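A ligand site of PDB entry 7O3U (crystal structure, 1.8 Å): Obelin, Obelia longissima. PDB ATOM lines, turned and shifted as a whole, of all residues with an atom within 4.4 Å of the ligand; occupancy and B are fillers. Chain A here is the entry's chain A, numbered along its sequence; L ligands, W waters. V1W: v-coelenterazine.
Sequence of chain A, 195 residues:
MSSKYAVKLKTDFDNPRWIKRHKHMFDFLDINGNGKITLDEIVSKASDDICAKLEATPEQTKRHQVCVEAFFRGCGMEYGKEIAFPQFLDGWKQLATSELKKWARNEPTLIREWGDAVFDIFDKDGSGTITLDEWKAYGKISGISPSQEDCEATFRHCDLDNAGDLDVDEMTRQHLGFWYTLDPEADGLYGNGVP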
ATOM      1  N   HIS A  22      15.725 -15.209  -6.833  1.00  0.00           N
ATOM      2  CA  HIS A  22      15.582 -14.193  -7.884  1.00  0.00           C
ATOM      3  C   HIS A  22      16.051 -14.703  -9.230  1.00  0.00           C
ATOM      4  O   HIS A  22      15.619 -14.170 -10.265  1.00  0.00           O
ATOM      5  CB  HIS A  22      16.313 -12.896  -7.509  1.00  0.00           C
ATOM      6  CG  HIS A  22      15.692 -12.180  -6.341  1.00  0.00           C
ATOM      7  ND1 HIS A  22      14.629 -11.305  -6.485  1.00  0.00           N
ATOM      8  CD2 HIS A  22      15.932 -12.263  -5.006  1.00  0.00           C
ATOM      9  CE1 HIS A  22      14.266 -10.862  -5.287  1.00  0.00           C
ATOM     10  NE2 HIS A  22      15.048 -11.408  -4.375  1.00  0.00           N
ATOM     11  N   MET A  25      12.891 -15.835 -10.690  1.00  0.00           N
ATOM     12  CA  MET A  25      12.027 -14.769 -11.174  1.00  0.00           C
ATOM     13  C   MET A  25      12.602 -14.081 -12.407  1.00  0.00           C
ATOM     14  O   MET A  25      11.849 -13.635 -13.278  1.00  0.00           O
ATOM     15  CB  MET A  25      11.794 -13.774 -10.042  1.00  0.00           C
ATOM     16  CG  MET A  25      11.007 -14.447  -8.865  1.00  0.00           C
ATOM     17  SD  MET A  25       9.356 -14.879  -9.380  1.00  0.00           S
ATOM     18  CE  MET A  25       8.597 -13.292  -9.721  1.00  0.00           C
ATOM     19  N   PHE A  28      11.722 -16.288 -15.262  1.00  0.00           N
ATOM     20  CA  PHE A  28      10.315 -16.026 -15.478  1.00  0.00           C
ATOM     21  C   PHE A  28      10.121 -14.760 -16.271  1.00  0.00           C
ATOM     22  O   PHE A  28       9.284 -14.743 -17.185  1.00  0.00           O
ATOM     23  CB  PHE A  28       9.623 -15.958 -14.100  1.00  0.00           C
ATOM     24  CG  PHE A  28       8.411 -15.076 -14.046  1.00  0.00           C
ATOM     25  CD1 PHE A  28       7.214 -15.475 -14.614  1.00  0.00           C
ATOM     26  CD2 PHE A  28       8.441 -13.895 -13.327  1.00  0.00           C
ATOM     27  CE1 PHE A  28       6.074 -14.661 -14.510  1.00  0.00           C
ATOM     28  CE2 PHE A  28       7.311 -13.087 -13.204  1.00  0.00           C
ATOM     29  CZ  PHE A  28       6.115 -13.464 -13.802  1.00  0.00           C
ATOM     30  N   LEU A  29      10.877 -13.680 -15.943  1.00  0.00           N
ATOM     31  CA  LEU A  29      10.778 -12.455 -16.753  1.00  0.00           C
ATOM     32  C   LEU A  29      11.440 -12.626 -18.122  1.00  0.00           C
ATOM     33  O   LEU A  29      10.994 -12.022 -19.100  1.00  0.00           O
ATOM     34  CB  LEU A  29      11.396 -11.274 -16.006  1.00  0.00           C
ATOM     35  CG  LEU A  29      10.661 -10.868 -14.737  1.00  0.00           C
ATOM     36  CD1 LEU A  29      11.474  -9.746 -14.041  1.00  0.00           C
ATOM     37  CD2 LEU A  29       9.236 -10.345 -15.026  1.00  0.00           C
ATOM     38  N   ILE A  42       9.064  -5.248 -19.188  1.00  0.00           N
ATOM     39  CA  ILE A  42       8.392  -5.349 -17.893  1.00  0.00           C
ATOM     40  C   ILE A  42       7.152  -4.460 -17.874  1.00  0.00           C
ATOM     41  O   ILE A  42       6.063  -4.861 -17.428  1.00  0.00           O
ATOM     42  CB  ILE A  42       9.380  -4.981 -16.779  1.00  0.00           C
ATOM     43  CG1 ILE A  42      10.180  -6.206 -16.313  1.00  0.00           C
ATOM     44  CG2 ILE A  42       8.631  -4.523 -15.527  1.00  0.00           C
ATOM     45  CD1 ILE A  42      10.996  -6.898 -17.367  1.00  0.00           C
ATOM     46  N   LYS A  45       4.397  -5.719 -19.970  1.00  0.00           N
ATOM     47  CA  LYS A  45       3.716  -6.793 -19.257  1.00  0.00           C
ATOM     48  C   LYS A  45       2.764  -6.219 -18.212  1.00  0.00           C
ATOM     49  O   LYS A  45       1.625  -6.695 -18.070  1.00  0.00           O
ATOM     50  CB  LYS A  45       4.745  -7.730 -18.618  1.00  0.00           C
ATOM     51  CG  LYS A  45       4.217  -8.870 -17.718  1.00  0.00           C
ATOM     52  CD  LYS A  45       5.429  -9.623 -17.100  1.00  0.00           C
ATOM     53  CE  LYS A  45       5.006 -10.706 -16.100  1.00  0.00           C
ATOM     54  NZ  LYS A  45       4.559 -11.973 -16.756  1.00  0.00           N
ATOM     55  N   ALA A  46       3.206  -5.159 -17.527  1.00  0.00           N
ATOM     56  CA  ALA A  46       2.355  -4.539 -16.500  1.00  0.00           C
ATOM     57  C   ALA A  46       1.110  -3.900 -17.100  1.00  0.00           C
ATOM     58  O   ALA A  46      -0.004  -4.189 -16.667  1.00  0.00           O
ATOM     59  CB  ALA A  46       3.136  -3.496 -15.712  1.00  0.00           C
ATOM     60  N   ILE A  50      -1.370  -6.938 -18.182  1.00  0.00           N
ATOM     61  CA  ILE A  50      -2.110  -7.133 -16.903  1.00  0.00           C
ATOM     62  C   ILE A  50      -3.211  -6.083 -16.705  1.00  0.00           C
ATOM     63  O   ILE A  50      -4.380  -6.471 -16.597  1.00  0.00           O
ATOM     64  CB  ILE A  50      -1.123  -7.187 -15.711  1.00  0.00           C
ATOM     65  CG1 ILE A  50      -0.301  -8.476 -15.723  1.00  0.00           C
ATOM     66  CG2 ILE A  50      -1.867  -7.011 -14.397  1.00  0.00           C
ATOM     67  CD1 ILE A  50       0.885  -8.436 -14.797  1.00  0.00           C
ATOM     68  N   VAL A  68       5.324  -0.014 -10.900  1.00  0.00           N
ATOM     69  CA  VAL A  68       6.214  -0.990 -11.526  1.00  0.00           C
ATOM     70  C   VAL A  68       7.484  -0.330 -12.000  1.00  0.00           C
ATOM     71  O   VAL A  68       8.586  -0.872 -11.798  1.00  0.00           O
ATOM     72  CB  VAL A  68       5.473  -1.688 -12.682  1.00  0.00           C
ATOM     73  CG1 VAL A  68       6.545  -2.534 -13.516  1.00  0.00           C
ATOM     74  CG2 VAL A  68       4.334  -2.512 -12.052  1.00  0.00           C
ATOM     75  N   PHE A  71       9.708   0.282  -8.983  1.00  0.00           N
ATOM     76  CA  PHE A  71      10.207  -0.926  -8.350  1.00  0.00           C
ATOM     77  C   PHE A  71      11.375  -1.472  -9.168  1.00  0.00           C
ATOM     78  O   PHE A  71      12.469  -1.709  -8.655  1.00  0.00           O
ATOM     79  CB  PHE A  71       9.096  -1.960  -8.276  1.00  0.00           C
ATOM     80  CG  PHE A  71       9.455  -3.227  -7.583  1.00  0.00           C
ATOM     81  CD1 PHE A  71       9.295  -3.363  -6.220  1.00  0.00           C
ATOM     82  CD2 PHE A  71       9.914  -4.325  -8.299  1.00  0.00           C
ATOM     83  CE1 PHE A  71       9.593  -4.568  -5.557  1.00  0.00           C
ATOM     84  CE2 PHE A  71      10.202  -5.524  -7.655  1.00  0.00           C
ATOM     85  CZ  PHE A  71      10.038  -5.665  -6.276  1.00  0.00           C
ATOM     86  N   PHE A  72      11.179  -1.595 -10.468  1.00  0.00           N
ATOM     87  CA  PHE A  72      12.286  -2.206 -11.222  1.00  0.00           C
ATOM     88  C   PHE A  72      13.428  -1.228 -11.501  1.00  0.00           C
ATOM     89  O   PHE A  72      14.569  -1.672 -11.669  1.00  0.00           O
ATOM     90  CB  PHE A  72      11.722  -2.847 -12.481  1.00  0.00           C
ATOM     91  CG  PHE A  72      10.942  -4.115 -12.154  1.00  0.00           C
ATOM     92  CD1 PHE A  72      11.619  -5.310 -11.893  1.00  0.00           C
ATOM     93  CD2 PHE A  72       9.547  -4.095 -12.086  1.00  0.00           C
ATOM     94  CE1 PHE A  72      10.944  -6.464 -11.548  1.00  0.00           C
ATOM     95  CE2 PHE A  72       8.846  -5.258 -11.762  1.00  0.00           C
ATOM     96  CZ  PHE A  72       9.583  -6.475 -11.514  1.00  0.00           C
ATOM     97  N   PHE A  88      21.219  -7.839 -12.759  1.00  0.00           N
ATOM     98  CA  PHE A  88      19.898  -7.857 -12.083  1.00  0.00           C
ATOM     99  C   PHE A  88      20.063  -8.193 -10.607  1.00  0.00           C
ATOM    100  O   PHE A  88      19.528  -7.504  -9.721  1.00  0.00           O
ATOM    101  CB  PHE A  88      19.000  -8.891 -12.758  1.00  0.00           C
ATOM    102  CG  PHE A  88      17.592  -8.991 -12.210  1.00  0.00           C
ATOM    103  CD1 PHE A  88      16.615  -8.078 -12.584  1.00  0.00           C
ATOM    104  CD2 PHE A  88      17.230 -10.046 -11.424  1.00  0.00           C
ATOM    105  CE1 PHE A  88      15.286  -8.202 -12.144  1.00  0.00           C
ATOM    106  CE2 PHE A  88      15.903 -10.181 -10.963  1.00  0.00           C
ATOM    107  CZ  PHE A  88      14.950  -9.252 -11.307  1.00  0.00           C
ATOM    108  N   TRP A  92      19.338  -6.074  -7.295  1.00  0.00           N
ATOM    109  CA  TRP A  92      18.406  -6.514  -6.253  1.00  0.00           C
ATOM    110  C   TRP A  92      18.989  -6.347  -4.850  1.00  0.00           C
ATOM    111  O   TRP A  92      18.236  -6.087  -3.890  1.00  0.00           O
ATOM    112  CB  TRP A  92      17.996  -7.970  -6.484  1.00  0.00           C
ATOM    113  CG  TRP A  92      16.596  -7.984  -6.958  1.00  0.00           C
ATOM    114  CD1 TRP A  92      16.183  -7.976  -8.252  1.00  0.00           C
ATOM    115  CD2 TRP A  92      15.408  -7.894  -6.153  1.00  0.00           C
ATOM    116  NE1 TRP A  92      14.803  -7.929  -8.315  1.00  0.00           N
ATOM    117  CE2 TRP A  92      14.303  -7.886  -7.039  1.00  0.00           C
ATOM    118  CE3 TRP A  92      15.168  -7.856  -4.770  1.00  0.00           C
ATOM    119  CZ2 TRP A  92      12.991  -7.838  -6.588  1.00  0.00           C
ATOM    120  CZ3 TRP A  92      13.866  -7.791  -4.329  1.00  0.00           C
ATOM    121  CH2 TRP A  92      12.789  -7.786  -5.246  1.00  0.00           C
ATOM    122  N   ILE A 111       7.406  -2.013  -2.702  1.00  0.00           N
ATOM    123  CA  ILE A 111       6.534  -3.164  -2.806  1.00  0.00           C
ATOM    124  C   ILE A 111       5.203  -2.875  -2.123  1.00  0.00           C
ATOM    125  O   ILE A 111       4.177  -3.337  -2.592  1.00  0.00           O
ATOM    126  CB  ILE A 111       7.210  -4.437  -2.247  1.00  0.00           C
ATOM    127  CG1 ILE A 111       6.428  -5.689  -2.576  1.00  0.00           C
ATOM    128  CG2 ILE A 111       7.274  -4.377  -0.718  1.00  0.00           C
ATOM    129  CD1 ILE A 111       6.418  -6.047  -4.074  1.00  0.00           C
ATOM    130  N   TRP A 114       3.354  -0.829  -4.846  1.00  0.00           N
ATOM    131  CA  TRP A 114       2.862  -1.682  -5.922  1.00  0.00           C
ATOM    132  C   TRP A 114       1.691  -2.522  -5.461  1.00  0.00           C
ATOM    133  O   TRP A 114       0.656  -2.628  -6.162  1.00  0.00           O
ATOM    134  CB  TRP A 114       4.049  -2.555  -6.415  1.00  0.00           C
ATOM    135  CG  TRP A 114       3.822  -3.405  -7.653  1.00  0.00           C
ATOM    136  CD1 TRP A 114       2.750  -3.428  -8.497  1.00  0.00           C
ATOM    137  CD2 TRP A 114       4.720  -4.386  -8.111  1.00  0.00           C
ATOM    138  NE1 TRP A 114       2.977  -4.323  -9.529  1.00  0.00           N
ATOM    139  CE2 TRP A 114       4.166  -4.963  -9.290  1.00  0.00           C
ATOM    140  CE3 TRP A 114       5.946  -4.852  -7.644  1.00  0.00           C
ATOM    141  CZ2 TRP A 114       4.827  -5.954 -10.005  1.00  0.00           C
ATOM    142  CZ3 TRP A 114       6.588  -5.864  -8.345  1.00  0.00           C
ATOM    143  CH2 TRP A 114       6.035  -6.401  -9.516  1.00  0.00           C
ATOM    144  N   GLY A 115       1.790  -3.112  -4.271  1.00  0.00           N
ATOM    145  CA  GLY A 115       0.677  -3.904  -3.762  1.00  0.00           C
ATOM    146  C   GLY A 115      -0.606  -3.103  -3.632  1.00  0.00           C
ATOM    147  O   GLY A 115      -1.691  -3.577  -3.963  1.00  0.00           O
ATOM    148  N   VAL A 118      -2.071  -2.805  -7.062  1.00  0.00           N
ATOM    149  CA  VAL A 118      -2.656  -4.027  -7.597  1.00  0.00           C
ATOM    150  C   VAL A 118      -3.996  -4.269  -6.932  1.00  0.00           C
ATOM    151  O   VAL A 118      -4.991  -4.574  -7.603  1.00  0.00           O
ATOM    152  CB  VAL A 118      -1.723  -5.217  -7.413  1.00  0.00           C
ATOM    153  CG1 VAL A 118      -2.475  -6.529  -7.693  1.00  0.00           C
ATOM    154  CG2 VAL A 118      -0.542  -5.077  -8.392  1.00  0.00           C
ATOM    155  N   PHE A 119      -4.030  -4.136  -5.600  1.00  0.00           N
ATOM    156  CA  PHE A 119      -5.269  -4.478  -4.895  1.00  0.00           C
ATOM    157  C   PHE A 119      -6.386  -3.526  -5.281  1.00  0.00           C
ATOM    158  O   PHE A 119      -7.557  -3.921  -5.307  1.00  0.00           O
ATOM    159  CB  PHE A 119      -5.054  -4.469  -3.379  1.00  0.00           C
ATOM    160  CG  PHE A 119      -4.574  -5.786  -2.831  1.00  0.00           C
ATOM    161  CD1 PHE A 119      -3.275  -6.219  -3.058  1.00  0.00           C
ATOM    162  CD2 PHE A 119      -5.404  -6.566  -2.035  1.00  0.00           C
ATOM    163  CE1 PHE A 119      -2.807  -7.426  -2.556  1.00  0.00           C
ATOM    164  CE2 PHE A 119      -4.936  -7.772  -1.533  1.00  0.00           C
ATOM    165  CZ  PHE A 119      -3.659  -8.209  -1.761  1.00  0.00           C
ATOM    166  N   TRP A 135      -7.429 -13.601  -6.911  1.00  0.00           N
ATOM    167  CA  TRP A 135      -5.999 -13.878  -6.919  1.00  0.00           C
ATOM    168  C   TRP A 135      -5.619 -14.854  -8.018  1.00  0.00           C
ATOM    169  O   TRP A 135      -4.674 -14.615  -8.768  1.00  0.00           O
ATOM    170  CB  TRP A 135      -5.534 -14.392  -5.552  1.00  0.00           C
ATOM    171  CG  TRP A 135      -4.044 -14.765  -5.492  1.00  0.00           C
ATOM    172  CD1 TRP A 135      -3.509 -15.997  -5.251  1.00  0.00           C
ATOM    173  CD2 TRP A 135      -2.915 -13.866  -5.663  1.00  0.00           C
ATOM    174  NE1 TRP A 135      -2.136 -15.934  -5.259  1.00  0.00           N
ATOM    175  CE2 TRP A 135      -1.739 -14.645  -5.510  1.00  0.00           C
ATOM    176  CE3 TRP A 135      -2.793 -12.494  -5.918  1.00  0.00           C
ATOM    177  CZ2 TRP A 135      -0.453 -14.086  -5.603  1.00  0.00           C
ATOM    178  CZ3 TRP A 135      -1.506 -11.941  -6.019  1.00  0.00           C
ATOM    179  CH2 TRP A 135      -0.361 -12.746  -5.864  1.00  0.00           C
ATOM    180  N   TYR A 138      -5.196 -13.047 -10.961  1.00  0.00           N
ATOM    181  CA  TYR A 138      -3.885 -12.408 -11.009  1.00  0.00           C
ATOM    182  C   TYR A 138      -2.782 -13.424 -11.245  1.00  0.00           C
ATOM    183  O   TYR A 138      -1.847 -13.178 -12.014  1.00  0.00           O
ATOM    184  CB  TYR A 138      -3.599 -11.609  -9.724  1.00  0.00           C
ATOM    185  CG  TYR A 138      -2.264 -10.874  -9.890  1.00  0.00           C
ATOM    186  CD1 TYR A 138      -2.168  -9.785 -10.745  1.00  0.00           C
ATOM    187  CD2 TYR A 138      -1.089 -11.347  -9.287  1.00  0.00           C
ATOM    188  CE1 TYR A 138      -0.959  -9.152 -10.967  1.00  0.00           C
ATOM    189  CE2 TYR A 138       0.144 -10.692  -9.510  1.00  0.00           C
ATOM    190  CZ  TYR A 138       0.188  -9.617 -10.362  1.00  0.00           C
ATOM    191  OH  TYR A 138       1.375  -8.961 -10.644  1.00  0.00           O
ATOM    192  N   ILE A 144       2.761 -15.223 -12.590  1.00  0.00           N
ATOM    193  CA  ILE A 144       3.646 -15.590 -11.495  1.00  0.00           C
ATOM    194  C   ILE A 144       3.209 -16.907 -10.850  1.00  0.00           C
ATOM    195  O   ILE A 144       4.038 -17.611 -10.254  1.00  0.00           O
ATOM    196  CB  ILE A 144       3.741 -14.450 -10.470  1.00  0.00           C
ATOM    197  CG1 ILE A 144       4.889 -14.685  -9.483  1.00  0.00           C
ATOM    198  CG2 ILE A 144       2.415 -14.276  -9.738  1.00  0.00           C
ATOM    199  CD1 ILE A 144       5.122 -13.475  -8.541  1.00  0.00           C
ATOM    200  N   VAL A 168      -4.041  -6.687   1.624  1.00  0.00           N
ATOM    201  CA  VAL A 168      -2.736  -6.272   1.114  1.00  0.00           C
ATOM    202  C   VAL A 168      -1.786  -5.994   2.277  1.00  0.00           C
ATOM    203  O   VAL A 168      -0.576  -6.136   2.120  1.00  0.00           O
ATOM    204  CB  VAL A 168      -2.859  -5.041   0.207  1.00  0.00           C
ATOM    205  CG1 VAL A 168      -3.624  -3.864   0.892  1.00  0.00           C
ATOM    206  CG2 VAL A 168      -1.490  -4.579  -0.279  1.00  0.00           C
ATOM    207  N   MET A 171      -0.170  -9.335   2.672  1.00  0.00           N
ATOM    208  CA  MET A 171       0.744  -9.687   1.567  1.00  0.00           C
ATOM    209  C   MET A 171       2.002  -8.852   1.629  1.00  0.00           C
ATOM    210  O   MET A 171       3.087  -9.307   1.271  1.00  0.00           O
ATOM    211  CB  MET A 171       0.033  -9.527   0.226  1.00  0.00           C
ATOM    212  CG  MET A 171       0.793 -10.182  -0.965  1.00  0.00           C
ATOM    213  SD  MET A 171       0.828 -11.922  -0.535  1.00  0.00           S
ATOM    214  CE  MET A 171       0.915 -12.630  -2.196  1.00  0.00           C
ATOM    215  N   THR A 172       1.880  -7.578   2.026  1.00  0.00           N
ATOM    216  CA  THR A 172       3.077  -6.733   2.108  1.00  0.00           C
ATOM    217  C   THR A 172       4.040  -7.261   3.161  1.00  0.00           C
ATOM    218  O   THR A 172       5.257  -7.318   2.928  1.00  0.00           O
ATOM    219  CB  THR A 172       2.691  -5.291   2.439  1.00  0.00           C
ATOM    220  OG1 THR A 172       1.879  -4.790   1.380  1.00  0.00           O
ATOM    221  CG2 THR A 172       3.913  -4.435   2.542  1.00  0.00           C
ATOM    222  N   HIS A 175       5.695 -10.295   1.780  1.00  0.00           N
ATOM    223  CA  HIS A 175       6.633  -9.978   0.705  1.00  0.00           C
ATOM    224  C   HIS A 175       7.962  -9.437   1.239  1.00  0.00           C
ATOM    225  O   HIS A 175       9.032  -9.708   0.665  1.00  0.00           O
ATOM    226  CB  HIS A 175       6.013  -8.951  -0.240  1.00  0.00           C
ATOM    227  CG  HIS A 175       5.219  -9.540  -1.346  1.00  0.00           C
ATOM    228  ND1 HIS A 175       4.312  -8.803  -2.080  1.00  0.00           N
ATOM    229  CD2 HIS A 175       5.236 -10.786  -1.895  1.00  0.00           C
ATOM    230  CE1 HIS A 175       3.816  -9.573  -3.042  1.00  0.00           C
ATOM    231  NE2 HIS A 175       4.335 -10.788  -2.930  1.00  0.00           N
ATOM    232  N   TRP A 179      10.963 -11.697  -0.348  1.00  0.00           N
ATOM    233  CA  TRP A 179      11.852 -11.179  -1.405  1.00  0.00           C
ATOM    234  C   TRP A 179      13.116 -10.519  -0.870  1.00  0.00           C
ATOM    235  O   TRP A 179      14.131 -10.498  -1.572  1.00  0.00           O
ATOM    236  CB  TRP A 179      11.139 -10.145  -2.281  1.00  0.00           C
ATOM    237  CG  TRP A 179       9.938 -10.633  -2.999  1.00  0.00           C
ATOM    238  CD1 TRP A 179       8.699 -10.079  -2.954  1.00  0.00           C
ATOM    239  CD2 TRP A 179       9.874 -11.704  -3.943  1.00  0.00           C
ATOM    240  NE1 TRP A 179       7.836 -10.776  -3.763  1.00  0.00           N
ATOM    241  CE2 TRP A 179       8.530 -11.774  -4.392  1.00  0.00           C
ATOM    242  CE3 TRP A 179      10.815 -12.619  -4.444  1.00  0.00           C
ATOM    243  CZ2 TRP A 179       8.100 -12.721  -5.311  1.00  0.00           C
ATOM    244  CZ3 TRP A 179      10.383 -13.555  -5.385  1.00  0.00           C
ATOM    245  CH2 TRP A 179       9.040 -13.613  -5.804  1.00  0.00           C
ATOM    246  N   TYR A 190       4.691 -18.504  -1.965  1.00  0.00           N
ATOM    247  CA  TYR A 190       4.107 -18.924  -3.229  1.00  0.00           C
ATOM    248  C   TYR A 190       4.147 -20.428  -3.378  1.00  0.00           C
ATOM    249  O   TYR A 190       4.364 -20.924  -4.484  1.00  0.00           O
ATOM    250  CB  TYR A 190       4.843 -18.270  -4.412  1.00  0.00           C
ATOM    251  CG  TYR A 190       4.700 -16.769  -4.504  1.00  0.00           C
ATOM    252  CD1 TYR A 190       5.478 -15.939  -3.732  1.00  0.00           C
ATOM    253  CD2 TYR A 190       3.763 -16.199  -5.357  1.00  0.00           C
ATOM    254  CE1 TYR A 190       5.360 -14.583  -3.812  1.00  0.00           C
ATOM    255  CE2 TYR A 190       3.609 -14.824  -5.431  1.00  0.00           C
ATOM    256  CZ  TYR A 190       4.427 -14.014  -4.651  1.00  0.00           C
ATOM    257  OH  TYR A 190       4.312 -12.630  -4.701  1.00  0.00           O
HETATM  258  C1  V1W L   1       4.716  -9.287  -7.100  1.00  0.00           C
HETATM  259  C10 V1W L   1       9.218 -10.091  -9.079  1.00  0.00           C
HETATM  260  C11 V1W L   1      11.305 -10.174  -7.858  1.00  0.00           C
HETATM  261  C12 V1W L   1      11.948 -10.492  -9.043  1.00  0.00           C
HETATM  262  C13 V1W L   1      11.237 -10.526 -10.201  1.00  0.00           C
HETATM  263  C14 V1W L   1       9.880 -10.382 -10.308  1.00  0.00           C
HETATM  264  C15 V1W L   1       5.032 -10.102 -11.758  1.00  0.00           C
HETATM  265  C16 V1W L   1       5.255  -8.890 -12.698  1.00  0.00           C
HETATM  266  C17 V1W L   1       4.069  -8.026 -13.092  1.00  0.00           C
HETATM  267  C18 V1W L   1       4.184  -6.967 -13.871  1.00  0.00           C
HETATM  268  C19 V1W L   1       5.548  -6.597 -14.401  1.00  0.00           C
HETATM  269  C2  V1W L   1       5.081  -9.713  -9.282  1.00  0.00           C
HETATM  270  C20 V1W L   1       6.589  -7.347 -14.039  1.00  0.00           C
HETATM  271  C21 V1W L   1       6.451  -8.577 -13.136  1.00  0.00           C
HETATM  272  C22 V1W L   1       2.647  -7.967  -7.762  1.00  0.00           C
HETATM  273  C23 V1W L   1       2.240  -7.709  -6.305  1.00  0.00           C
HETATM  274  C24 V1W L   1       2.960  -6.887  -5.574  1.00  0.00           C
HETATM  275  C25 V1W L   1       2.518  -6.632  -4.120  1.00  0.00           C
HETATM  276  C26 V1W L   1       1.451  -7.237  -3.631  1.00  0.00           C
HETATM  277  C27 V1W L   1       0.642  -8.181  -4.499  1.00  0.00           C
HETATM  278  C28 V1W L   1       1.015  -8.417  -5.750  1.00  0.00           C
HETATM  279  C3  V1W L   1       3.404  -9.299  -7.827  1.00  0.00           C
HETATM  280  C4  V1W L   1       7.125  -9.675  -7.918  1.00  0.00           C
HETATM  281  C5  V1W L   1       7.851  -9.952  -9.071  1.00  0.00           C
HETATM  282  C6  V1W L   1       5.771  -9.964 -10.422  1.00  0.00           C
HETATM  283  C7  V1W L   1       7.824  -9.559  -6.748  1.00  0.00           C
HETATM  284  C8  V1W L   1       9.203  -9.693  -6.671  1.00  0.00           C
HETATM  285  C9  V1W L   1       9.908 -10.021  -7.877  1.00  0.00           C
HETATM  286  N1  V1W L   1       5.780  -9.574  -8.104  1.00  0.00           N
HETATM  287  N2  V1W L   1       3.673  -9.506  -9.192  1.00  0.00           N
HETATM  288  N3  V1W L   1       7.148 -10.074 -10.262  1.00  0.00           N
HETATM  289  O1  V1W L   1      13.346 -10.691  -9.077  1.00  0.00           O
HETATM  290  O2  V1W L   1       4.989  -9.163  -5.751  1.00  0.00           O
HETATM  291  O3  V1W L   1       2.656 -10.388  -7.390  1.00  0.00           O
HETATM  292  O4  V1W L   1       3.524 -11.185  -6.591  1.00  0.00           O
HETATM  293  O5  V1W L   1       1.081  -7.000  -2.292  1.00  0.00           O
HETATM  294  O   HOH W   1       1.414  -6.447 -11.783  1.00  0.00           O
HETATM  295  O   HOH W   2       2.852  -5.423  -1.081  1.00  0.00           O
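Merely in contact with the ligand: Met 25 (3.2 Å), Leu 29 (3.8 Å), Ile 42 (3.5 Å), Lys 45 (3.9 Å), Ile 50 (3.6 Å), Phe 72 (3.8 Å), Phe 88 (3.1 Å), Ile 111 (3.8 Å), Trp 114 (3.5 Å), Gly 115 (3.3 Å), Phe 119 (3.9 Å), Ile 144 (3.4 Å), Met 171 (3.5 Å) and Trp 179 (3.2 Å).
The backbone NH (N) of Ile 50 is in hydrogen-bond range of the backbone carbonyl oxygen (O) of Lys 45. O of Trp 179 is in hydrogen-bond range of NE2 of His 22. OH of Tyr 190 is in hydrogen-bond range of NE2 of His 175, at 2.6 Å.
Water W2 lies within hydrogen-bond range of an oxygen (O5) of the ligand (2.7 Å), the side-chain hydroxyl of Thr 172 (2.7 Å) and the backbone carbonyl oxygen of Ile 111 (2.9 Å). Water W1 lies within hydrogen-bond range of the side-chain hydroxyl of Tyr 138 and the indole nitrogen of Trp 114.
O1 of the ligand is in hydrogen-bond range of NE1 of Trp 92, 3.2 Å away. An oxygen (O2) of the ligand sits close to a ring nitrogen (NE2) of His 175. ND1 of His 22 is in hydrogen-bond range of O1 of the ligand (3.0 Å). The side-chain hydroxyl (OH) of Tyr 190 lies within hydrogen-bond range of an oxygen (O4) of the ligand, 2.5 Å away. OH of Tyr 138 is in hydrogen-bond range of N2 of the ligand, at 2.8 Å.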
